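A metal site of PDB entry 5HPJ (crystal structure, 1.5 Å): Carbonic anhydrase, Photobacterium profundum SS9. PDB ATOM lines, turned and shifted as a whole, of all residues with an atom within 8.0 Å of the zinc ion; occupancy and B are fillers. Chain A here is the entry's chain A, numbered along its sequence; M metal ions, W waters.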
ATOM      1  N   TYR A   4       3.201 -18.001   4.940  1.00  0.00           N
ATOM      2  CA  TYR A   4       2.313 -18.077   6.093  1.00  0.00           C
ATOM      3  C   TYR A   4       2.348 -19.410   6.819  1.00  0.00           C
ATOM      4  O   TYR A   4       2.350 -19.464   8.043  1.00  0.00           O
ATOM      5  CB  TYR A   4       0.886 -17.675   5.690  1.00  0.00           C
ATOM      6  CG  TYR A   4       0.834 -16.179   5.580  1.00  0.00           C
ATOM      7  CD1 TYR A   4       0.525 -15.405   6.682  1.00  0.00           C
ATOM      8  CD2 TYR A   4       1.208 -15.541   4.400  1.00  0.00           C
ATOM      9  CE1 TYR A   4       0.536 -14.035   6.604  1.00  0.00           C
ATOM     10  CE2 TYR A   4       1.208 -14.187   4.307  1.00  0.00           C
ATOM     11  CZ  TYR A   4       0.900 -13.425   5.423  1.00  0.00           C
ATOM     12  OH  TYR A   4       0.935 -12.041   5.331  1.00  0.00           O
ATOM     13  N   THR A  27       0.945  -6.270  15.626  1.00  0.00           N
ATOM     14  CA  THR A  27      -0.354  -6.315  14.960  1.00  0.00           C
ATOM     15  C   THR A  27      -0.398  -7.663  14.220  1.00  0.00           C
ATOM     16  O   THR A  27       0.639  -8.124  13.741  1.00  0.00           O
ATOM     17  CB  THR A  27      -0.471  -5.133  13.990  1.00  0.00           C
ATOM     18  OG1 THR A  27      -0.239  -3.921  14.722  1.00  0.00           O
ATOM     19  CG2 THR A  27      -1.838  -5.066  13.319  1.00  0.00           C
ATOM     20  N   HIS A  58       2.759 -12.575  -1.737  1.00  0.00           N
ATOM     21  CA  HIS A  58       2.315 -12.425  -0.343  1.00  0.00           C
ATOM     22  C   HIS A  58       0.940 -11.784  -0.231  1.00  0.00           C
ATOM     23  O   HIS A  58       0.185 -12.053   0.705  1.00  0.00           O
ATOM     24  CB  HIS A  58       3.298 -11.564   0.416  1.00  0.00           C
ATOM     25  CG  HIS A  58       4.679 -12.150   0.467  1.00  0.00           C
ATOM     26  ND1 HIS A  58       5.799 -11.479   0.025  1.00  0.00           N
ATOM     27  CD2 HIS A  58       5.114 -13.332   0.938  1.00  0.00           C
ATOM     28  CE1 HIS A  58       6.858 -12.248   0.205  1.00  0.00           C
ATOM     29  NE2 HIS A  58       6.472 -13.374   0.769  1.00  0.00           N
ATOM     30  N   THR A  59       0.655 -10.901  -1.191  1.00  0.00           N
ATOM     31  CA  THR A  59      -0.592 -10.161  -1.230  1.00  0.00           C
ATOM     32  C   THR A  59      -0.793  -9.616  -2.634  1.00  0.00           C
ATOM     33  O   THR A  59       0.077  -9.744  -3.495  1.00  0.00           O
ATOM     34  CB  THR A  59      -0.577  -8.987  -0.234  1.00  0.00           C
ATOM     35  OG1 THR A  59      -1.864  -8.364  -0.189  1.00  0.00           O
ATOM     36  CG2 THR A  59       0.462  -7.939  -0.639  1.00  0.00           C
ATOM     37  N   GLN A  81       0.975   2.508  -0.772  1.00  0.00           N
ATOM     38  CA  GLN A  81       0.309   1.372  -1.402  1.00  0.00           C
ATOM     39  C   GLN A  81      -0.830   0.949  -0.493  1.00  0.00           C
ATOM     40  O   GLN A  81      -0.839   1.278   0.693  1.00  0.00           O
ATOM     41  CB  GLN A  81       1.254   0.164  -1.594  1.00  0.00           C
ATOM     42  CG  GLN A  81       2.129  -0.172  -0.396  1.00  0.00           C
ATOM     43  CD  GLN A  81       1.618  -1.276   0.504  1.00  0.00           C
ATOM     44  OE1 GLN A  81       0.499  -1.777   0.348  1.00  0.00           O
ATOM     45  NE2 GLN A  81       2.455  -1.670   1.453  1.00  0.00           N
ATOM     46  N   PHE A  82      -1.784   0.210  -1.046  1.00  0.00           N
ATOM     47  CA  PHE A  82      -2.680  -0.556  -0.216  1.00  0.00           C
ATOM     48  C   PHE A  82      -2.716  -1.990  -0.677  1.00  0.00           C
ATOM     49  O   PHE A  82      -2.398  -2.287  -1.824  1.00  0.00           O
ATOM     50  CB  PHE A  82      -4.082   0.058  -0.087  1.00  0.00           C
ATOM     51  CG  PHE A  82      -4.862   0.163  -1.379  1.00  0.00           C
ATOM     52  CD1 PHE A  82      -5.788  -0.796  -1.712  1.00  0.00           C
ATOM     53  CD2 PHE A  82      -4.729   1.273  -2.197  1.00  0.00           C
ATOM     54  CE1 PHE A  82      -6.546  -0.683  -2.860  1.00  0.00           C
ATOM     55  CE2 PHE A  82      -5.483   1.388  -3.358  1.00  0.00           C
ATOM     56  CZ  PHE A  82      -6.391   0.404  -3.683  1.00  0.00           C
ATOM     57  N   HIS A  83      -3.064  -2.889   0.223  1.00  0.00           N
ATOM     58  CA  HIS A  83      -3.078  -4.315  -0.116  1.00  0.00           C
ATOM     59  C   HIS A  83      -4.092  -5.045   0.745  1.00  0.00           C
ATOM     60  O   HIS A  83      -4.714  -4.460   1.631  1.00  0.00           O
ATOM     61  CB  HIS A  83      -1.686  -4.911   0.064  1.00  0.00           C
ATOM     62  CG  HIS A  83      -1.237  -4.895   1.483  1.00  0.00           C
ATOM     63  ND1 HIS A  83      -0.495  -3.862   2.001  1.00  0.00           N
ATOM     64  CD2 HIS A  83      -1.515  -5.727   2.517  1.00  0.00           C
ATOM     65  CE1 HIS A  83      -0.309  -4.068   3.288  1.00  0.00           C
ATOM     66  NE2 HIS A  83      -0.931  -5.191   3.631  1.00  0.00           N
ATOM     67  N   PHE A  84      -4.236  -6.351   0.503  1.00  0.00           N
ATOM     68  CA  PHE A  84      -5.354  -7.105   1.049  1.00  0.00           C
ATOM     69  C   PHE A  84      -4.936  -8.363   1.763  1.00  0.00           C
ATOM     70  O   PHE A  84      -3.913  -8.975   1.452  1.00  0.00           O
ATOM     71  CB  PHE A  84      -6.324  -7.488  -0.076  1.00  0.00           C
ATOM     72  CG  PHE A  84      -6.944  -6.320  -0.764  1.00  0.00           C
ATOM     73  CD1 PHE A  84      -8.068  -5.704  -0.234  1.00  0.00           C
ATOM     74  CD2 PHE A  84      -6.426  -5.831  -1.952  1.00  0.00           C
ATOM     75  CE1 PHE A  84      -8.656  -4.624  -0.862  1.00  0.00           C
ATOM     76  CE2 PHE A  84      -7.007  -4.736  -2.576  1.00  0.00           C
ATOM     77  CZ  PHE A  84      -8.126  -4.139  -2.033  1.00  0.00           C
ATOM     78  N   HIS A  85      -5.772  -8.746   2.734  1.00  0.00           N
ATOM     79  CA  HIS A  85      -5.648 -10.007   3.440  1.00  0.00           C
ATOM     80  C   HIS A  85      -6.994 -10.707   3.432  1.00  0.00           C
ATOM     81  O   HIS A  85      -8.026 -10.075   3.676  1.00  0.00           O
ATOM     82  CB  HIS A  85      -5.176  -9.796   4.876  1.00  0.00           C
ATOM     83  CG  HIS A  85      -3.846  -9.109   4.983  1.00  0.00           C
ATOM     84  ND1 HIS A  85      -2.665  -9.808   5.086  1.00  0.00           N
ATOM     85  CD2 HIS A  85      -3.507  -7.800   4.998  1.00  0.00           C
ATOM     86  CE1 HIS A  85      -1.657  -8.954   5.151  1.00  0.00           C
ATOM     87  NE2 HIS A  85      -2.142  -7.733   5.102  1.00  0.00           N
ATOM     88  N   GLU A  89      -7.032  -9.849   9.294  1.00  0.00           N
ATOM     89  CA  GLU A  89      -6.005 -10.070  10.283  1.00  0.00           C
ATOM     90  C   GLU A  89      -6.474  -9.566  11.629  1.00  0.00           C
ATOM     91  O   GLU A  89      -6.531 -10.330  12.600  1.00  0.00           O
ATOM     92  CB  GLU A  89      -4.695  -9.376   9.888  1.00  0.00           C
ATOM     93  CG  GLU A  89      -4.198  -9.819   8.541  1.00  0.00           C
ATOM     94  CD  GLU A  89      -2.736  -9.540   8.363  1.00  0.00           C
ATOM     95  OE1 GLU A  89      -2.378  -8.341   8.227  1.00  0.00           O
ATOM     96  OE2 GLU A  89      -1.947 -10.490   8.439  1.00  0.00           O
ATOM     97  N   ASN A  90      -6.818  -8.284  11.718  1.00  0.00           N
ATOM     98  CA  ASN A  90      -7.446  -7.772  12.941  1.00  0.00           C
ATOM     99  C   ASN A  90      -8.885  -8.299  13.037  1.00  0.00           C
ATOM    100  O   ASN A  90      -9.495  -8.646  12.006  1.00  0.00           O
ATOM    101  CB  ASN A  90      -7.429  -6.242  12.972  1.00  0.00           C
ATOM    102  CG  ASN A  90      -6.026  -5.683  12.984  1.00  0.00           C
ATOM    103  OD1 ASN A  90      -5.286  -5.856  13.964  1.00  0.00           O
ATOM    104  ND2 ASN A  90      -5.638  -5.028  11.895  1.00  0.00           N
ATOM    105  N   GLU A 100      -9.676  -7.761   4.566  1.00  0.00           N
ATOM    106  CA  GLU A 100      -9.191  -6.520   5.206  1.00  0.00           C
ATOM    107  C   GLU A 100      -8.203  -5.824   4.263  1.00  0.00           C
ATOM    108  O   GLU A 100      -7.320  -6.482   3.711  1.00  0.00           O
ATOM    109  CB  GLU A 100      -8.532  -6.854   6.550  1.00  0.00           C
ATOM    110  CG  GLU A 100      -7.993  -5.633   7.294  1.00  0.00           C
ATOM    111  CD  GLU A 100      -7.418  -5.946   8.669  1.00  0.00           C
ATOM    112  OE1 GLU A 100      -7.593  -7.089   9.136  1.00  0.00           O
ATOM    113  OE2 GLU A 100      -6.792  -5.061   9.288  1.00  0.00           O
ATOM    114  N   ALA A 101      -8.354  -4.506   4.086  1.00  0.00           N
ATOM    115  CA  ALA A 101      -7.422  -3.688   3.309  1.00  0.00           C
ATOM    116  C   ALA A 101      -6.538  -2.899   4.257  1.00  0.00           C
ATOM    117  O   ALA A 101      -7.037  -2.377   5.258  1.00  0.00           O
ATOM    118  CB  ALA A 101      -8.162  -2.761   2.400  1.00  0.00           C
ATOM    119  N   HIS A 102      -5.245  -2.835   3.939  1.00  0.00           N
ATOM    120  CA  HIS A 102      -4.288  -1.998   4.648  1.00  0.00           C
ATOM    121  C   HIS A 102      -3.770  -0.923   3.729  1.00  0.00           C
ATOM    122  O   HIS A 102      -3.142  -1.225   2.707  1.00  0.00           O
ATOM    123  CB  HIS A 102      -3.134  -2.828   5.153  1.00  0.00           C
ATOM    124  CG  HIS A 102      -3.532  -3.786   6.230  1.00  0.00           C
ATOM    125  ND1 HIS A 102      -2.826  -4.948   6.494  1.00  0.00           N
ATOM    126  CD2 HIS A 102      -4.580  -3.779   7.080  1.00  0.00           C
ATOM    127  CE1 HIS A 102      -3.428  -5.580   7.492  1.00  0.00           C
ATOM    128  NE2 HIS A 102      -4.491  -4.890   7.860  1.00  0.00           N
ATOM    129  N   PHE A 103      -4.061   0.321   4.090  1.00  0.00           N
ATOM    130  CA  PHE A 103      -3.566   1.491   3.372  1.00  0.00           C
ATOM    131  C   PHE A 103      -2.303   1.947   4.127  1.00  0.00           C
ATOM    132  O   PHE A 103      -2.376   2.449   5.261  1.00  0.00           O
ATOM    133  CB  PHE A 103      -4.634   2.580   3.376  1.00  0.00           C
ATOM    134  CG  PHE A 103      -5.837   2.252   2.537  1.00  0.00           C
ATOM    135  CD1 PHE A 103      -6.844   1.448   3.024  1.00  0.00           C
ATOM    136  CD2 PHE A 103      -5.955   2.758   1.272  1.00  0.00           C
ATOM    137  CE1 PHE A 103      -7.951   1.135   2.263  1.00  0.00           C
ATOM    138  CE2 PHE A 103      -7.054   2.439   0.498  1.00  0.00           C
ATOM    139  CZ  PHE A 103      -8.045   1.643   0.998  1.00  0.00           C
ATOM    140  N   VAL A 104      -1.150   1.738   3.515  1.00  0.00           N
ATOM    141  CA  VAL A 104       0.122   1.904   4.191  1.00  0.00           C
ATOM    142  C   VAL A 104       0.736   3.220   3.779  1.00  0.00           C
ATOM    143  O   VAL A 104       0.936   3.454   2.578  1.00  0.00           O
ATOM    144  CB  VAL A 104       1.077   0.742   3.852  1.00  0.00           C
ATOM    145  CG1 VAL A 104       2.419   0.910   4.587  1.00  0.00           C
ATOM    146  CG2 VAL A 104       0.427  -0.615   4.199  1.00  0.00           C
ATOM    147  N   VAL A 114      -0.720   2.895   9.219  1.00  0.00           N
ATOM    148  CA  VAL A 114      -1.632   2.062   8.456  1.00  0.00           C
ATOM    149  C   VAL A 114      -3.067   2.409   8.807  1.00  0.00           C
ATOM    150  O   VAL A 114      -3.425   2.455   9.987  1.00  0.00           O
ATOM    151  CB  VAL A 114      -1.364   0.566   8.707  1.00  0.00           C
ATOM    152  CG1 VAL A 114      -2.292  -0.295   7.836  1.00  0.00           C
ATOM    153  CG2 VAL A 114       0.093   0.239   8.443  1.00  0.00           C
ATOM    154  N   ALA A 116      -6.625   0.718   8.309  1.00  0.00           N
ATOM    155  CA  ALA A 116      -7.216  -0.571   7.988  1.00  0.00           C
ATOM    156  C   ALA A 116      -8.706  -0.417   7.771  1.00  0.00           C
ATOM    157  O   ALA A 116      -9.389   0.288   8.505  1.00  0.00           O
ATOM    158  CB  ALA A 116      -6.942  -1.591   9.113  1.00  0.00           C
ATOM    159  N   SER A 167       2.544  -2.793  14.809  1.00  0.00           N
ATOM    160  CA  SER A 167       3.648  -3.214  13.952  1.00  0.00           C
ATOM    161  C   SER A 167       3.154  -3.472  12.545  1.00  0.00           C
ATOM    162  O   SER A 167       1.954  -3.546  12.317  1.00  0.00           O
ATOM    163  CB  SER A 167       4.255  -4.509  14.482  1.00  0.00           C
ATOM    164  OG  SER A 167       3.425  -5.648  14.254  1.00  0.00           O
ATOM    165  N   LEU A 168       4.081  -3.693  11.644  1.00  0.00           N
ATOM    166  CA  LEU A 168       3.737  -4.330  10.371  1.00  0.00           C
ATOM    167  C   LEU A 168       3.317  -5.740  10.664  1.00  0.00           C
ATOM    168  O   LEU A 168       3.820  -6.353  11.611  1.00  0.00           O
ATOM    169  CB  LEU A 168       4.928  -4.323   9.424  1.00  0.00           C
ATOM    170  CG  LEU A 168       5.415  -2.919   9.060  1.00  0.00           C
ATOM    171  CD1 LEU A 168       6.639  -3.067   8.174  1.00  0.00           C
ATOM    172  CD2 LEU A 168       4.335  -2.074   8.377  1.00  0.00           C
ATOM    173  N   THR A 169       2.384  -6.275   9.874  1.00  0.00           N
ATOM    174  CA  THR A 169       1.896  -7.640  10.087  1.00  0.00           C
ATOM    175  C   THR A 169       2.638  -8.627   9.208  1.00  0.00           C
ATOM    176  O   THR A 169       2.342  -9.822   9.229  1.00  0.00           O
ATOM    177  CB  THR A 169       0.391  -7.778   9.813  1.00  0.00           C
ATOM    178  OG1 THR A 169       0.159  -7.651   8.407  1.00  0.00           O
ATOM    179  CG2 THR A 169      -0.444  -6.746  10.569  1.00  0.00           C
ATOM    180  N   THR A 170       3.617  -8.138   8.453  1.00  0.00           N
ATOM    181  CA  THR A 170       4.474  -8.983   7.630  1.00  0.00           C
ATOM    182  C   THR A 170       5.934  -8.654   7.929  1.00  0.00           C
ATOM    183  O   THR A 170       6.236  -7.553   8.388  1.00  0.00           O
ATOM    184  CB  THR A 170       4.204  -8.726   6.147  1.00  0.00           C
ATOM    185  OG1 THR A 170       4.258  -7.314   5.909  1.00  0.00           O
ATOM    186  CG2 THR A 170       2.857  -9.264   5.765  1.00  0.00           C
ATOM    187  N   TRP A 179      -1.670   2.438  14.017  1.00  0.00           N
ATOM    188  CA  TRP A 179      -2.792   1.746  13.415  1.00  0.00           C
ATOM    189  C   TRP A 179      -4.100   2.488  13.667  1.00  0.00           C
ATOM    190  O   TRP A 179      -4.433   2.823  14.801  1.00  0.00           O
ATOM    191  CB  TRP A 179      -2.892   0.299  13.933  1.00  0.00           C
ATOM    192  CG  TRP A 179      -1.904  -0.569  13.213  1.00  0.00           C
ATOM    193  CD1 TRP A 179      -0.562  -0.680  13.462  1.00  0.00           C
ATOM    194  CD2 TRP A 179      -2.175  -1.411  12.094  1.00  0.00           C
ATOM    195  NE1 TRP A 179       0.007  -1.545  12.555  1.00  0.00           N
ATOM    196  CE2 TRP A 179      -0.952  -2.001  11.705  1.00  0.00           C
ATOM    197  CE3 TRP A 179      -3.331  -1.730  11.377  1.00  0.00           C
ATOM    198  CZ2 TRP A 179      -0.867  -2.900  10.644  1.00  0.00           C
ATOM    199  CZ3 TRP A 179      -3.228  -2.607  10.326  1.00  0.00           C
ATOM    200  CH2 TRP A 179      -2.022  -3.196   9.977  1.00  0.00           C
ATOM    201  N   ASN A 203      -3.592 -15.435   3.794  1.00  0.00           N
ATOM    202  CA  ASN A 203      -2.448 -14.583   4.112  1.00  0.00           C
ATOM    203  C   ASN A 203      -2.715 -13.686   5.305  1.00  0.00           C
ATOM    204  O   ASN A 203      -2.265 -12.524   5.369  1.00  0.00           O
ATOM    205  CB  ASN A 203      -2.034 -13.783   2.872  1.00  0.00           C
ATOM    206  CG  ASN A 203      -3.056 -12.779   2.442  1.00  0.00           C
ATOM    207  OD1 ASN A 203      -4.190 -12.804   2.861  1.00  0.00           O
ATOM    208  ND2 ASN A 203      -2.654 -11.895   1.555  1.00  0.00           N
HETATM  209 ZN    ZN M   1      -1.344  -5.886   5.457  1.00  0.00          ZN
HETATM  210  O   HOH W   1       0.311  -5.973   6.385  1.00  0.00           O
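The zinc ion is bound by water W1, a ring nitrogen (NE2) of His 83, a ring nitrogen (ND1) of His 102 and a ring nitrogen (NE2) of His 85.
A ring nitrogen (ND1) of His 85 sits close to the side-chain carboxylate of Glu 89, at 3.5 Å. The backbone carbonyl oxygen (O) of Glu 100 is in hydrogen-bond range of the backbone NH (N) of His 85, at 2.9 Å. A ring nitrogen (NE2) of His 102 is in hydrogen-bond range of the side-chain carboxylate (OE2) of Glu 100 (2.7 Å). OE1 of Glu 100 is in hydrogen-bond range of N of Glu 89. OG1 of Thr 169 is in hydrogen-bond range of OE1 of Glu 89. The side-chain amide oxygen of Gln 81 sits at hydrogen-bond distance from a ring nitrogen (ND1) of His 83. A ring nitrogen (ND1) of His 85 lies within hydrogen-bond range of the backbone carbonyl oxygen of Asn 203 (2.8 Å).
Glu 89 touches the zinc ion. Thr 169 touches the zinc ion (OG1 to ZN, 3.8 Å). Five residues have an atom within 4 Å of the zinc ion: His 83, His 85, Glu 89, His 102 and Thr 169. Along chain A the residues within 4 Å of the zinc ion span positions 83 to 169.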
